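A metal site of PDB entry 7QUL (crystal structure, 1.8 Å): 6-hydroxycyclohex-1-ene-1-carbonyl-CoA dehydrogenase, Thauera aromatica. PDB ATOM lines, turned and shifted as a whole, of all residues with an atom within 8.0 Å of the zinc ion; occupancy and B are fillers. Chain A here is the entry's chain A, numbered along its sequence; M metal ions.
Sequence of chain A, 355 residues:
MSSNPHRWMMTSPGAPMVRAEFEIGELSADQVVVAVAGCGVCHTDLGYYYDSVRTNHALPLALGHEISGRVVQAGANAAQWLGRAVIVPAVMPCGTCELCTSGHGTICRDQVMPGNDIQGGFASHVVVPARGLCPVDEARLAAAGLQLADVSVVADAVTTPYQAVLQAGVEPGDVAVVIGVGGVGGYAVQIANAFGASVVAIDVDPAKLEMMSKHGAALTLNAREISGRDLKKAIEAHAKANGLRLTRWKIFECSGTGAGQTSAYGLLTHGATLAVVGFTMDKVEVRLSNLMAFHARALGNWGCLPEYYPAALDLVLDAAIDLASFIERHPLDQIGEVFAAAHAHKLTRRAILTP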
ATOM      1  N   GLY A  40     -20.324   3.960  10.302  1.00  0.00           N
ATOM      2  CA  GLY A  40     -19.130   3.523   9.553  1.00  0.00           C
ATOM      3  C   GLY A  40     -17.832   3.896  10.237  1.00  0.00           C
ATOM      4  O   GLY A  40     -17.786   4.908  10.965  1.00  0.00           O
ATOM      5  N   VAL A  41     -16.796   3.077  10.013  1.00  0.00           N
ATOM      6  CA  VAL A  41     -15.409   3.311  10.490  1.00  0.00           C
ATOM      7  C   VAL A  41     -14.590   3.824   9.314  1.00  0.00           C
ATOM      8  O   VAL A  41     -14.482   3.081   8.330  1.00  0.00           O
ATOM      9  CB  VAL A  41     -14.821   2.028  11.077  1.00  0.00           C
ATOM     10  CG1 VAL A  41     -13.380   2.255  11.520  1.00  0.00           C
ATOM     11  CG2 VAL A  41     -15.711   1.529  12.218  1.00  0.00           C
ATOM     12  N   CYS A  42     -14.027   5.019   9.431  1.00  0.00           N
ATOM     13  CA  CYS A  42     -13.535   5.788   8.265  1.00  0.00           C
ATOM     14  C   CYS A  42     -12.044   6.063   8.449  1.00  0.00           C
ATOM     15  O   CYS A  42     -11.557   6.134   9.611  1.00  0.00           O
ATOM     16  CB  CYS A  42     -14.297   7.097   8.130  1.00  0.00           C
ATOM     17  SG  CYS A  42     -13.803   8.089   6.696  1.00  0.00           S
ATOM     18  N   HIS A  43     -11.339   6.247   7.337  1.00  0.00           N
ATOM     19  CA  HIS A  43      -9.920   6.676   7.379  1.00  0.00           C
ATOM     20  C   HIS A  43      -9.815   7.980   8.200  1.00  0.00           C
ATOM     21  O   HIS A  43      -8.770   8.172   8.901  1.00  0.00           O
ATOM     22  CB  HIS A  43      -9.334   6.662   5.950  1.00  0.00           C
ATOM     23  CG  HIS A  43      -9.203   5.267   5.417  1.00  0.00           C
ATOM     24  ND1 HIS A  43      -8.947   4.173   6.254  1.00  0.00           N
ATOM     25  CD2 HIS A  43      -9.260   4.776   4.164  1.00  0.00           C
ATOM     26  CE1 HIS A  43      -8.863   3.078   5.529  1.00  0.00           C
ATOM     27  NE2 HIS A  43      -9.052   3.413   4.244  1.00  0.00           N
ATOM     28  N   THR A  44     -10.855   8.810   8.166  1.00  0.00           N
ATOM     29  CA  THR A  44     -10.854  10.105   8.902  1.00  0.00           C
ATOM     30  C   THR A  44     -10.799   9.819  10.418  1.00  0.00           C
ATOM     31  O   THR A  44     -10.129  10.573  11.134  1.00  0.00           O
ATOM     32  CB  THR A  44     -12.016  10.984   8.413  1.00  0.00           C
ATOM     33  OG1 THR A  44     -11.826  11.300   7.030  1.00  0.00           O
ATOM     34  CG2 THR A  44     -12.161  12.255   9.232  1.00  0.00           C
ATOM     35  N   ASP A  45     -11.554   8.829  10.913  1.00  0.00           N
ATOM     36  CA  ASP A  45     -11.552   8.436  12.342  1.00  0.00           C
ATOM     37  C   ASP A  45     -10.153   7.950  12.717  1.00  0.00           C
ATOM     38  O   ASP A  45      -9.609   8.334  13.779  1.00  0.00           O
ATOM     39  CB  ASP A  45     -12.627   7.389  12.612  1.00  0.00           C
ATOM     40  CG  ASP A  45     -14.026   7.815  12.191  1.00  0.00           C
ATOM     41  OD1 ASP A  45     -14.503   8.842  12.673  1.00  0.00           O
ATOM     42  OD2 ASP A  45     -14.606   7.137  11.374  1.00  0.00           O
ATOM     43  N   GLY A  64     -16.711   9.058  14.727  1.00  0.00           N
ATOM     44  CA  GLY A  64     -17.784   8.449  13.933  1.00  0.00           C
ATOM     45  C   GLY A  64     -18.626   9.519  13.277  1.00  0.00           C
ATOM     46  O   GLY A  64     -19.239  10.323  14.002  1.00  0.00           O
ATOM     47  N   HIS A  65     -18.662   9.514  11.943  1.00  0.00           N
ATOM     48  CA  HIS A  65     -19.391  10.546  11.153  1.00  0.00           C
ATOM     49  C   HIS A  65     -20.189   9.930  10.009  1.00  0.00           C
ATOM     50  O   HIS A  65     -20.571  10.683   9.133  1.00  0.00           O
ATOM     51  CB  HIS A  65     -18.413  11.598  10.602  1.00  0.00           C
ATOM     52  CG  HIS A  65     -17.389  11.040   9.682  1.00  0.00           C
ATOM     53  ND1 HIS A  65     -16.100  10.780  10.111  1.00  0.00           N
ATOM     54  CD2 HIS A  65     -17.448  10.702   8.370  1.00  0.00           C
ATOM     55  CE1 HIS A  65     -15.405  10.281   9.084  1.00  0.00           C
ATOM     56  NE2 HIS A  65     -16.228  10.211   8.003  1.00  0.00           N
ATOM     57  N   GLU A  66     -20.425   8.612  10.015  1.00  0.00           N
ATOM     58  CA  GLU A  66     -21.150   7.930   8.925  1.00  0.00           C
ATOM     59  C   GLU A  66     -22.328   7.228   9.570  1.00  0.00           C
ATOM     60  O   GLU A  66     -22.206   6.007   9.819  1.00  0.00           O
ATOM     61  CB  GLU A  66     -20.191   6.983   8.161  1.00  0.00           C
ATOM     62  CG  GLU A  66     -19.085   7.714   7.462  1.00  0.00           C
ATOM     63  CD  GLU A  66     -18.026   6.888   6.760  1.00  0.00           C
ATOM     64  OE1 GLU A  66     -18.220   5.618   6.686  1.00  0.00           O
ATOM     65  OE2 GLU A  66     -17.012   7.517   6.273  1.00  0.00           O
ATOM     66  N   ALA A  90     -22.339  13.638   6.770  1.00  0.00           N
ATOM     67  CA  ALA A  90     -20.976  13.610   7.356  1.00  0.00           C
ATOM     68  C   ALA A  90     -20.468  15.040   7.568  1.00  0.00           C
ATOM     69  O   ALA A  90     -19.728  15.312   8.544  1.00  0.00           O
ATOM     70  CB  ALA A  90     -20.088  12.843   6.409  1.00  0.00           C
ATOM     71  N   MET A 113     -18.926  18.858  11.298  1.00  0.00           N
ATOM     72  CA  MET A 113     -18.861  17.394  11.176  1.00  0.00           C
ATOM     73  C   MET A 113     -19.004  16.697  12.528  1.00  0.00           C
ATOM     74  O   MET A 113     -18.316  17.017  13.502  1.00  0.00           O
ATOM     75  CB  MET A 113     -17.507  17.141  10.521  1.00  0.00           C
ATOM     76  CG  MET A 113     -17.026  15.760  10.435  1.00  0.00           C
ATOM     77  SD  MET A 113     -15.504  16.070   9.560  1.00  0.00           S
ATOM     78  CE  MET A 113     -14.339  14.910  10.258  1.00  0.00           C
ATOM     79  N   VAL A 153     -23.214   4.015   5.824  1.00  0.00           N
ATOM     80  CA  VAL A 153     -22.028   4.318   4.963  1.00  0.00           C
ATOM     81  C   VAL A 153     -22.437   5.073   3.701  1.00  0.00           C
ATOM     82  O   VAL A 153     -21.564   5.488   2.916  1.00  0.00           O
ATOM     83  CB  VAL A 153     -21.244   3.030   4.650  1.00  0.00           C
ATOM     84  CG1 VAL A 153     -20.743   2.407   5.943  1.00  0.00           C
ATOM     85  CG2 VAL A 153     -22.086   2.035   3.861  1.00  0.00           C
ATOM     86  N   ALA A 155     -23.420   8.020   4.111  1.00  0.00           N
ATOM     87  CA  ALA A 155     -22.701   9.231   4.578  1.00  0.00           C
ATOM     88  C   ALA A 155     -21.209   9.041   4.301  1.00  0.00           C
ATOM     89  O   ALA A 155     -20.629   8.043   4.794  1.00  0.00           O
ATOM     90  CB  ALA A 155     -22.993   9.497   6.024  1.00  0.00           C
ATOM     91  N   ASP A 156     -20.637   9.968   3.527  1.00  0.00           N
ATOM     92  CA  ASP A 156     -19.223   9.993   3.080  1.00  0.00           C
ATOM     93  C   ASP A 156     -18.945   8.858   2.082  1.00  0.00           C
ATOM     94  O   ASP A 156     -18.574   9.169   0.961  1.00  0.00           O
ATOM     95  CB  ASP A 156     -18.269   9.980   4.282  1.00  0.00           C
ATOM     96  CG  ASP A 156     -16.828  10.254   3.889  1.00  0.00           C
ATOM     97  OD1 ASP A 156     -16.593  10.709   2.738  1.00  0.00           O
ATOM     98  OD2 ASP A 156     -15.932  10.040   4.754  1.00  0.00           O
ATOM     99  N   ALA A 157     -19.031   7.572   2.464  1.00  0.00           N
ATOM    100  CA  ALA A 157     -18.397   6.493   1.651  1.00  0.00           C
ATOM    101  C   ALA A 157     -19.073   6.421   0.278  1.00  0.00           C
ATOM    102  O   ALA A 157     -18.343   6.288  -0.719  1.00  0.00           O
ATOM    103  CB  ALA A 157     -18.385   5.150   2.335  1.00  0.00           C
ATOM    104  N   THR A 160     -19.506  10.977  -1.103  1.00  0.00           N
ATOM    105  CA  THR A 160     -18.257  11.624  -1.559  1.00  0.00           C
ATOM    106  C   THR A 160     -18.028  11.320  -3.040  1.00  0.00           C
ATOM    107  O   THR A 160     -17.901  12.251  -3.850  1.00  0.00           O
ATOM    108  CB  THR A 160     -17.087  11.316  -0.610  1.00  0.00           C
ATOM    109  OG1 THR A 160     -17.375  12.005   0.624  1.00  0.00           O
ATOM    110  CG2 THR A 160     -15.757  11.777  -1.162  1.00  0.00           C
ATOM    111  N   VAL A 184     -14.295   4.302  -0.925  1.00  0.00           N
ATOM    112  CA  VAL A 184     -14.859   5.390  -1.767  1.00  0.00           C
ATOM    113  C   VAL A 184     -14.734   5.022  -3.252  1.00  0.00           C
ATOM    114  O   VAL A 184     -15.691   5.235  -4.008  1.00  0.00           O
ATOM    115  CB  VAL A 184     -14.183   6.727  -1.421  1.00  0.00           C
ATOM    116  CG1 VAL A 184     -14.065   7.633  -2.632  1.00  0.00           C
ATOM    117  CG2 VAL A 184     -14.886   7.431  -0.270  1.00  0.00           C
ATOM    118  N   ARG A 350     -16.093  -2.292   4.628  1.00  0.00           N
ATOM    119  CA  ARG A 350     -16.220  -1.145   5.551  1.00  0.00           C
ATOM    120  C   ARG A 350     -16.914  -1.641   6.822  1.00  0.00           C
ATOM    121  O   ARG A 350     -18.033  -2.188   6.705  1.00  0.00           O
ATOM    122  CB  ARG A 350     -17.018  -0.013   4.912  1.00  0.00           C
ATOM    123  CG  ARG A 350     -16.802   1.328   5.600  1.00  0.00           C
ATOM    124  CD  ARG A 350     -17.384   2.434   4.732  1.00  0.00           C
ATOM    125  NE  ARG A 350     -16.843   3.753   5.041  1.00  0.00           N
ATOM    126  CZ  ARG A 350     -15.676   4.224   4.620  1.00  0.00           C
ATOM    127  NH1 ARG A 350     -14.868   3.514   3.849  1.00  0.00           N
ATOM    128  NH2 ARG A 350     -15.326   5.459   4.970  1.00  0.00           N
HETATM  129 ZN    ZN M   1     -15.925   8.961   6.439  1.00  0.00          ZN
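The backbone NH of Gly 40 is in hydrogen-bond range of the backbone carbonyl oxygen of Glu 66 (2.8 Å).
The side-chain sulfur (SG) of Cys 42 lies close to the backbone NH (N) of Thr 44.
OD2 of Asp 45 is in hydrogen-bond range of N of Cys 42, 2.9 Å away.
NE of Arg 350 is in salt-bridge range of OE1 of Glu 66 (2.8 Å).
The side-chain sulfur (SG) of Cys 42 sits close to the guanidinium group (NH2) of Arg 350, at 3.5 Å.
The side-chain carboxylate of Asp 156 lies within hydrogen-bond range of the side-chain hydroxyl of Thr 160, 2.6 Å away.
Residues that only touch the zinc ion: Arg 350.
Within 4 Å of the zinc ion: Cys 42, His 65, Glu 66, Asp 156 and Arg 350.
The nearest printed residue that does not touch the zinc ion is Thr 44 (4.8 Å).
The zinc ion is bound by OE2 of Glu 66 (1.8 Å), OD2 of Asp 156 (2.0 Å), NE2 of His 65 (2.0 Å) and SG of Cys 42 (2.3 Å).
The zinc ion has four donor atoms within binding distance.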
